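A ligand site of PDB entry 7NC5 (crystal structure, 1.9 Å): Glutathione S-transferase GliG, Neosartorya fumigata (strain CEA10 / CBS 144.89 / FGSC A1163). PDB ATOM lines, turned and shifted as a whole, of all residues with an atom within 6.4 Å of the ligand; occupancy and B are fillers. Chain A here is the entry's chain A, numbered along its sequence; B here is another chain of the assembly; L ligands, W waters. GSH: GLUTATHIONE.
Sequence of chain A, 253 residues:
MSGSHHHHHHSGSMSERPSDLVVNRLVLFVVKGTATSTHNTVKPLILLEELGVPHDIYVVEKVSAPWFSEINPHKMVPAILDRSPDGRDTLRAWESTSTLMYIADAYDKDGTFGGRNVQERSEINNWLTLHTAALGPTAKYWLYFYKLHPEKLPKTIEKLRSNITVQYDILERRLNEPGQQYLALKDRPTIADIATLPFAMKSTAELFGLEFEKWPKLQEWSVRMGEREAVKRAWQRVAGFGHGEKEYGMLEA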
ATOM      1  N   VAL A  31     -10.626  26.991   5.745  1.00  0.00           N
ATOM      2  CA  VAL A  31      -9.159  27.215   5.700  1.00  0.00           C
ATOM      3  C   VAL A  31      -8.856  28.216   4.582  1.00  0.00           C
ATOM      4  O   VAL A  31      -9.801  28.592   3.843  1.00  0.00           O
ATOM      5  CB  VAL A  31      -8.364  25.900   5.528  1.00  0.00           C
ATOM      6  CG1 VAL A  31      -8.463  25.030   6.766  1.00  0.00           C
ATOM      7  CG2 VAL A  31      -8.775  25.128   4.283  1.00  0.00           C
ATOM      8  N   THR A  36      -7.731  23.437  -4.234  1.00  0.00           N
ATOM      9  CA  THR A  36      -7.910  22.084  -3.636  1.00  0.00           C
ATOM     10  C   THR A  36      -8.278  22.166  -2.142  1.00  0.00           C
ATOM     11  O   THR A  36      -8.222  21.110  -1.492  1.00  0.00           O
ATOM     12  CB  THR A  36      -6.657  21.219  -3.823  1.00  0.00           C
ATOM     13  OG1 THR A  36      -5.584  21.802  -3.090  1.00  0.00           O
ATOM     14  CG2 THR A  36      -6.262  21.063  -5.281  1.00  0.00           C
ATOM     15  N   SER A  37      -8.657  23.329  -1.608  1.00  0.00           N
ATOM     16  CA  SER A  37      -8.991  23.494  -0.167  1.00  0.00           C
ATOM     17  C   SER A  37     -10.448  23.933   0.044  1.00  0.00           C
ATOM     18  O   SER A  37     -10.819  24.128   1.223  1.00  0.00           O
ATOM     19  CB  SER A  37      -8.026  24.450   0.512  1.00  0.00           C
ATOM     20  OG  SER A  37      -8.359  25.810   0.222  1.00  0.00           O
ATOM     21  N   THR A  38     -11.243  24.041  -1.022  1.00  0.00           N
ATOM     22  CA  THR A  38     -12.566  24.725  -0.999  1.00  0.00           C
ATOM     23  C   THR A  38     -13.716  23.831  -1.481  1.00  0.00           C
ATOM     24  O   THR A  38     -14.870  24.287  -1.391  1.00  0.00           O
ATOM     25  CB  THR A  38     -12.514  26.012  -1.835  1.00  0.00           C
ATOM     26  OG1 THR A  38     -12.184  25.657  -3.182  1.00  0.00           O
ATOM     27  CG2 THR A  38     -11.519  27.020  -1.299  1.00  0.00           C
ATOM     28  N   ASN A  40     -15.087  21.125  -0.347  1.00  0.00           N
ATOM     29  CA  ASN A  40     -15.979  20.636   0.735  1.00  0.00           C
ATOM     30  C   ASN A  40     -16.609  21.821   1.481  1.00  0.00           C
ATOM     31  O   ASN A  40     -17.819  21.760   1.751  1.00  0.00           O
ATOM     32  CB  ASN A  40     -15.242  19.657   1.647  1.00  0.00           C
ATOM     33  CG  ASN A  40     -15.056  18.298   1.004  1.00  0.00           C
ATOM     34  OD1 ASN A  40     -16.014  17.699   0.511  1.00  0.00           O
ATOM     35  ND2 ASN A  40     -13.827  17.804   0.977  1.00  0.00           N
ATOM     36  N   THR A  41     -15.835  22.867   1.776  1.00  0.00           N
ATOM     37  CA  THR A  41     -16.314  24.063   2.535  1.00  0.00           C
ATOM     38  C   THR A  41     -17.323  24.854   1.701  1.00  0.00           C
ATOM     39  O   THR A  41     -18.227  25.453   2.309  1.00  0.00           O
ATOM     40  CB  THR A  41     -15.159  24.953   3.009  1.00  0.00           C
ATOM     41  OG1 THR A  41     -14.349  25.281   1.872  1.00  0.00           O
ATOM     42  CG2 THR A  41     -14.314  24.292   4.074  1.00  0.00           C
ATOM     43  N   LYS A  43     -19.701  23.746  -0.023  1.00  0.00           N
ATOM     44  CA  LYS A  43     -21.010  23.028  -0.002  1.00  0.00           C
ATOM     45  C   LYS A  43     -21.983  23.704   0.956  1.00  0.00           C
ATOM     46  O   LYS A  43     -23.044  24.151   0.530  1.00  0.00           O
ATOM     47  CB  LYS A  43     -20.804  21.544   0.325  1.00  0.00           C
ATOM     48  CG  LYS A  43     -20.066  20.751  -0.740  1.00  0.00           C
ATOM     49  CD  LYS A  43     -19.764  19.340  -0.308  1.00  0.00           C
ATOM     50  CE  LYS A  43     -18.978  18.553  -1.334  1.00  0.00           C
ATOM     51  NZ  LYS A  43     -18.877  17.122  -0.968  1.00  0.00           N
ATOM     52  N   VAL A  60      -9.452  28.845   9.913  1.00  0.00           N
ATOM     53  CA  VAL A  60      -8.630  28.015  10.837  1.00  0.00           C
ATOM     54  C   VAL A  60      -7.201  27.952  10.292  1.00  0.00           C
ATOM     55  O   VAL A  60      -7.041  27.563   9.118  1.00  0.00           O
ATOM     56  CB  VAL A  60      -9.237  26.610  11.016  1.00  0.00           C
ATOM     57  CG1 VAL A  60      -8.400  25.734  11.945  1.00  0.00           C
ATOM     58  CG2 VAL A  60     -10.672  26.675  11.518  1.00  0.00           C
ATOM     59  N   GLU A  61      -6.213  28.342  11.095  1.00  0.00           N
ATOM     60  CA  GLU A  61      -4.778  28.305  10.707  1.00  0.00           C
ATOM     61  C   GLU A  61      -4.293  26.844  10.733  1.00  0.00           C
ATOM     62  O   GLU A  61      -3.641  26.433   9.760  1.00  0.00           O
ATOM     63  CB  GLU A  61      -3.909  29.160  11.633  1.00  0.00           C
ATOM     64  CG  GLU A  61      -2.447  29.166  11.230  1.00  0.00           C
ATOM     65  CD  GLU A  61      -1.536  30.031  12.078  1.00  0.00           C
ATOM     66  OE1 GLU A  61      -0.346  30.135  11.739  1.00  0.00           O
ATOM     67  OE2 GLU A  61      -2.017  30.584  13.094  1.00  0.00           O
ATOM     68  N   VAL A  63      -5.865  22.994  11.655  1.00  0.00           N
ATOM     69  CA  VAL A  63      -6.976  22.048  11.987  1.00  0.00           C
ATOM     70  C   VAL A  63      -6.474  21.016  13.003  1.00  0.00           C
ATOM     71  O   VAL A  63      -7.320  20.310  13.581  1.00  0.00           O
ATOM     72  CB  VAL A  63      -7.552  21.355  10.730  1.00  0.00           C
ATOM     73  CG1 VAL A  63      -8.210  22.358   9.794  1.00  0.00           C
ATOM     74  CG2 VAL A  63      -6.509  20.528   9.981  1.00  0.00           C
ATOM     75  N   PHE A  68      -9.821  23.042  18.076  1.00  0.00           N
ATOM     76  CA  PHE A  68     -10.621  22.728  16.865  1.00  0.00           C
ATOM     77  C   PHE A  68     -11.123  21.280  16.916  1.00  0.00           C
ATOM     78  O   PHE A  68     -12.239  21.039  16.419  1.00  0.00           O
ATOM     79  CB  PHE A  68      -9.846  22.994  15.570  1.00  0.00           C
ATOM     80  CG  PHE A  68     -10.681  22.835  14.333  1.00  0.00           C
ATOM     81  CD1 PHE A  68     -11.749  23.695  14.084  1.00  0.00           C
ATOM     82  CD2 PHE A  68     -10.452  21.797  13.437  1.00  0.00           C
ATOM     83  CE1 PHE A  68     -12.537  23.528  12.955  1.00  0.00           C
ATOM     84  CE2 PHE A  68     -11.243  21.642  12.313  1.00  0.00           C
ATOM     85  CZ  PHE A  68     -12.283  22.509  12.079  1.00  0.00           C
ATOM     86  N   HIS A  74     -12.681  14.886  13.756  1.00  0.00           N
ATOM     87  CA  HIS A  74     -12.074  14.435  12.484  1.00  0.00           C
ATOM     88  C   HIS A  74     -11.059  15.482  11.973  1.00  0.00           C
ATOM     89  O   HIS A  74     -10.370  15.186  10.986  1.00  0.00           O
ATOM     90  CB  HIS A  74     -13.174  14.120  11.465  1.00  0.00           C
ATOM     91  CG  HIS A  74     -12.774  13.125  10.430  1.00  0.00           C
ATOM     92  ND1 HIS A  74     -13.531  12.893   9.297  1.00  0.00           N
ATOM     93  CD2 HIS A  74     -11.701  12.305  10.337  1.00  0.00           C
ATOM     94  CE1 HIS A  74     -12.949  11.962   8.561  1.00  0.00           C
ATOM     95  NE2 HIS A  74     -11.818  11.593   9.171  1.00  0.00           N
ATOM     96  N   LYS A  75     -10.976  16.645  12.630  1.00  0.00           N
ATOM     97  CA  LYS A  75      -9.910  17.672  12.436  1.00  0.00           C
ATOM     98  C   LYS A  75      -9.873  18.129  10.977  1.00  0.00           C
ATOM     99  O   LYS A  75      -8.776  18.164  10.385  1.00  0.00           O
ATOM    100  CB  LYS A  75      -8.559  17.102  12.895  1.00  0.00           C
ATOM    101  CG  LYS A  75      -8.514  16.627  14.337  1.00  0.00           C
ATOM    102  CD  LYS A  75      -7.182  16.029  14.747  1.00  0.00           C
ATOM    103  CE  LYS A  75      -7.212  15.433  16.132  1.00  0.00           C
ATOM    104  NZ  LYS A  75      -5.879  14.943  16.545  1.00  0.00           N
ATOM    105  N   MET A  76     -11.037  18.465  10.411  1.00  0.00           N
ATOM    106  CA  MET A  76     -11.154  18.950   9.007  1.00  0.00           C
ATOM    107  C   MET A  76     -12.231  20.026   8.922  1.00  0.00           C
ATOM    108  O   MET A  76     -13.070  20.125   9.841  1.00  0.00           O
ATOM    109  CB  MET A  76     -11.490  17.801   8.062  1.00  0.00           C
ATOM    110  CG  MET A  76     -10.363  16.806   7.891  1.00  0.00           C
ATOM    111  SD  MET A  76     -10.664  15.590   6.595  1.00  0.00           S
ATOM    112  CE  MET A  76     -12.215  14.877   7.155  1.00  0.00           C
ATOM    113  N   VAL A  77     -12.186  20.813   7.838  1.00  0.00           N
ATOM    114  CA  VAL A  77     -13.246  21.787   7.456  1.00  0.00           C
ATOM    115  C   VAL A  77     -14.015  21.202   6.271  1.00  0.00           C
ATOM    116  O   VAL A  77     -13.446  20.426   5.496  1.00  0.00           O
ATOM    117  CB  VAL A  77     -12.645  23.181   7.139  1.00  0.00           C
ATOM    118  CG1 VAL A  77     -12.034  23.807   8.385  1.00  0.00           C
ATOM    119  CG2 VAL A  77     -11.632  23.148   6.010  1.00  0.00           C
ATOM    120  N   PRO A  78     -15.320  21.510   6.107  1.00  0.00           N
ATOM    121  CA  PRO A  78     -16.020  22.455   6.965  1.00  0.00           C
ATOM    122  C   PRO A  78     -16.447  21.888   8.332  1.00  0.00           C
ATOM    123  O   PRO A  78     -16.614  20.696   8.476  1.00  0.00           O
ATOM    124  CB  PRO A  78     -17.283  22.790   6.150  1.00  0.00           C
ATOM    125  CG  PRO A  78     -17.556  21.514   5.374  1.00  0.00           C
ATOM    126  CD  PRO A  78     -16.189  20.958   5.059  1.00  0.00           C
ATOM    127  N   TRP A  94     -20.298  18.816  11.519  1.00  0.00           N
ATOM    128  CA  TRP A  94     -19.000  18.547  10.859  1.00  0.00           C
ATOM    129  C   TRP A  94     -19.144  17.319   9.955  1.00  0.00           C
ATOM    130  O   TRP A  94     -20.016  16.471  10.239  1.00  0.00           O
ATOM    131  CB  TRP A  94     -17.864  18.399  11.878  1.00  0.00           C
ATOM    132  CG  TRP A  94     -18.237  17.670  13.136  1.00  0.00           C
ATOM    133  CD1 TRP A  94     -18.688  18.209  14.302  1.00  0.00           C
ATOM    134  CD2 TRP A  94     -18.150  16.250  13.362  1.00  0.00           C
ATOM    135  NE1 TRP A  94     -18.897  17.229  15.231  1.00  0.00           N
ATOM    136  CE2 TRP A  94     -18.575  16.015  14.684  1.00  0.00           C
ATOM    137  CE3 TRP A  94     -17.760  15.160  12.577  1.00  0.00           C
ATOM    138  CZ2 TRP A  94     -18.631  14.733  15.239  1.00  0.00           C
ATOM    139  CZ3 TRP A  94     -17.810  13.896  13.127  1.00  0.00           C
ATOM    140  CH2 TRP A  94     -18.236  13.690  14.436  1.00  0.00           C
ATOM    141  N   GLU A  95     -18.288  17.240   8.924  1.00  0.00           N
ATOM    142  CA  GLU A  95     -18.506  16.511   7.653  1.00  0.00           C
ATOM    143  C   GLU A  95     -19.435  17.354   6.783  1.00  0.00           C
ATOM    144  O   GLU A  95     -20.542  17.686   7.245  1.00  0.00           O
ATOM    145  CB  GLU A  95     -19.086  15.105   7.863  1.00  0.00           C
ATOM    146  CG  GLU A  95     -18.076  14.106   8.387  1.00  0.00           C
ATOM    147  CD  GLU A  95     -16.918  13.871   7.437  1.00  0.00           C
ATOM    148  OE1 GLU A  95     -17.170  13.672   6.226  1.00  0.00           O
ATOM    149  OE2 GLU A  95     -15.758  13.908   7.900  1.00  0.00           O
ATOM    150  N   SER A  96     -18.992  17.696   5.563  1.00  0.00           N
ATOM    151  CA  SER A  96     -19.715  18.585   4.612  1.00  0.00           C
ATOM    152  C   SER A  96     -21.179  18.140   4.466  1.00  0.00           C
ATOM    153  O   SER A  96     -22.057  19.012   4.532  1.00  0.00           O
ATOM    154  CB  SER A  96     -19.013  18.637   3.278  1.00  0.00           C
ATOM    155  OG  SER A  96     -18.894  17.351   2.712  1.00  0.00           O
ATOM    156  N   THR A  97     -21.427  16.839   4.296  1.00  0.00           N
ATOM    157  CA  THR A  97     -22.805  16.293   4.110  1.00  0.00           C
ATOM    158  C   THR A  97     -23.635  16.614   5.364  1.00  0.00           C
ATOM    159  O   THR A  97     -24.810  16.991   5.200  1.00  0.00           O
ATOM    160  CB  THR A  97     -22.790  14.806   3.732  1.00  0.00           C
ATOM    161  OG1 THR A  97     -22.398  14.706   2.361  1.00  0.00           O
ATOM    162  CG2 THR A  97     -24.128  14.138   3.913  1.00  0.00           C
ATOM    163  N   LYS A 140     -11.235  12.139  -2.598  1.00  0.00           N
ATOM    164  CA  LYS A 140     -10.343  12.515  -1.458  1.00  0.00           C
ATOM    165  C   LYS A 140      -9.115  11.602  -1.439  1.00  0.00           C
ATOM    166  O   LYS A 140      -8.005  12.120  -1.257  1.00  0.00           O
ATOM    167  CB  LYS A 140     -11.096  12.446  -0.123  1.00  0.00           C
ATOM    168  CG  LYS A 140     -10.269  12.829   1.098  1.00  0.00           C
ATOM    169  CD  LYS A 140     -11.103  13.184   2.310  1.00  0.00           C
ATOM    170  CE  LYS A 140     -10.297  13.307   3.583  1.00  0.00           C
ATOM    171  NZ  LYS A 140      -9.338  14.434   3.530  1.00  0.00           N
ATOM    172  N   ALA B 133     -18.704   8.515   5.261  1.00  0.00           N
ATOM    173  CA  ALA B 133     -17.633   9.201   4.492  1.00  0.00           C
ATOM    174  C   ALA B 133     -16.247   8.600   4.785  1.00  0.00           C
ATOM    175  O   ALA B 133     -15.431   8.549   3.856  1.00  0.00           O
ATOM    176  CB  ALA B 133     -17.648  10.681   4.798  1.00  0.00           C
ATOM    177  N   ALA B 134     -15.990   8.184   6.032  1.00  0.00           N
ATOM    178  CA  ALA B 134     -14.649   7.786   6.522  1.00  0.00           C
ATOM    179  C   ALA B 134     -14.556   6.263   6.685  1.00  0.00           C
ATOM    180  O   ALA B 134     -14.074   5.609   5.739  1.00  0.00           O
ATOM    181  CB  ALA B 134     -14.325   8.529   7.801  1.00  0.00           C
HETATM  182  N1  GSH L   1     -15.151  14.024   4.420  1.00  0.00           N
HETATM  183  CA1 GSH L   1     -14.864  15.456   4.683  1.00  0.00           C
HETATM  184  C1  GSH L   1     -16.048  16.309   4.228  1.00  0.00           C
HETATM  185  O11 GSH L   1     -16.686  15.915   3.229  1.00  0.00           O
HETATM  186  O12 GSH L   1     -16.297  17.346   4.886  1.00  0.00           O
HETATM  187  CB1 GSH L   1     -13.580  15.890   3.981  1.00  0.00           C
HETATM  188  CG1 GSH L   1     -13.214  17.345   4.220  1.00  0.00           C
HETATM  189  CD1 GSH L   1     -11.780  17.646   3.845  1.00  0.00           C
HETATM  190  OE1 GSH L   1     -11.165  16.955   3.036  1.00  0.00           O
HETATM  191  N2  GSH L   1     -11.218  18.713   4.439  1.00  0.00           N
HETATM  192  CA2 GSH L   1      -9.875  19.183   4.159  1.00  0.00           C
HETATM  193  C2  GSH L   1      -9.177  19.788   5.379  1.00  0.00           C
HETATM  194  O2  GSH L   1      -9.850  20.060   6.375  1.00  0.00           O
HETATM  195  CB2 GSH L   1      -9.881  20.184   3.012  1.00  0.00           C
HETATM  196  SG2 GSH L   1      -8.492  21.336   2.975  1.00  0.00           S
HETATM  197  N3  GSH L   1      -7.861  19.985   5.303  1.00  0.00           N
HETATM  198  CA3 GSH L   1      -7.168  20.781   6.298  1.00  0.00           C
HETATM  199  C3  GSH L   1      -5.796  21.260   5.832  1.00  0.00           C
HETATM  200  O31 GSH L   1      -4.926  20.389   5.635  1.00  0.00           O
HETATM  201  O32 GSH L   1      -5.635  22.497   5.688  1.00  0.00           O
HETATM  202  O   HOH W   1     -15.278  12.884   1.893  1.00  0.00           O
HETATM  203  O   HOH W   2      -4.607  23.343   8.676  1.00  0.00           O
HETATM  204  O   HOH W   3     -19.494  14.435   4.189  1.00  0.00           O
HETATM  205  O   HOH W   4     -15.752  18.309   7.461  1.00  0.00           O
HETATM  206  O   HOH W   5     -12.061  19.721   0.761  1.00  0.00           O
HETATM  207  O   HOH W   6     -13.108  11.967   5.133  1.00  0.00           O
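Residues that only touch the ligand: Met 76 (3.1 Å), Pro 78 (3.6 Å), Val 63 (3.8 Å), Ser 37 (3.8 Å) and Val 31 (3.9 Å). Hydrophobic or aromatic side chains within 4 Å of the ligand: Val 31, Val 63, Met 76, Val 77 and Pro 78. Of the 23 residues printed, 10 come within 4 Å of the ligand. The nearest printed residue that does not touch the ligand is Ala 133 of chain B (4.2 Å).
Water W4 lies within hydrogen-bond range of O of Pro 78 (2.7 Å), O12 of the ligand (2.8 Å) and N of Glu 95 (3.1 Å). Water W2 lies within hydrogen-bond range of the backbone NH (N) of Val 63 (3.3 Å), an oxygen (O32) of the ligand (3.3 Å) and the backbone carbonyl oxygen (O) of Glu 61 (3.4 Å). Water W3 lies within hydrogen-bond range of the backbone NH (N) of Thr 97, the side-chain carboxylate (OE1) of Glu 95, an oxygen (O11) of the ligand and the side-chain hydroxyl (OG) of Ser 96.
The side-chain sulfur (SD) of Met 76 lies within hydrogen-bond range of the side-chain amino group (NZ) of Lys 140 (3.5 Å). The side-chain carboxylate (OE2) of Glu 95 lies within hydrogen-bond range of a ring nitrogen (ND1) of His 74 (2.8 Å). OD1 of Asn 40 lies within hydrogen-bond range of NZ of Lys 43 (3.3 Å).
N2 of the ligand sits at hydrogen-bond distance from O of Val 77 (3.0 Å). An oxygen (O11) of the ligand lies within hydrogen-bond range of the side-chain hydroxyl of Ser 96. OE1 of Glu 95 lies within salt-bridge range of N1 of the ligand (2.7 Å). The side-chain amino group (NZ) of Lys 140 sits at hydrogen-bond distance from an oxygen (OE1) of the ligand, at 3.2 Å. N of Ser 96 lies within hydrogen-bond range of O12 of the ligand, 2.8 Å away. The backbone NH (N) of Val 77 is in hydrogen-bond range of an oxygen (O2) of the ligand, at 2.9 Å. The side-chain amide oxygen (OD1) of Asn 40 sits close to an oxygen (O11) of the ligand (3.3 Å).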
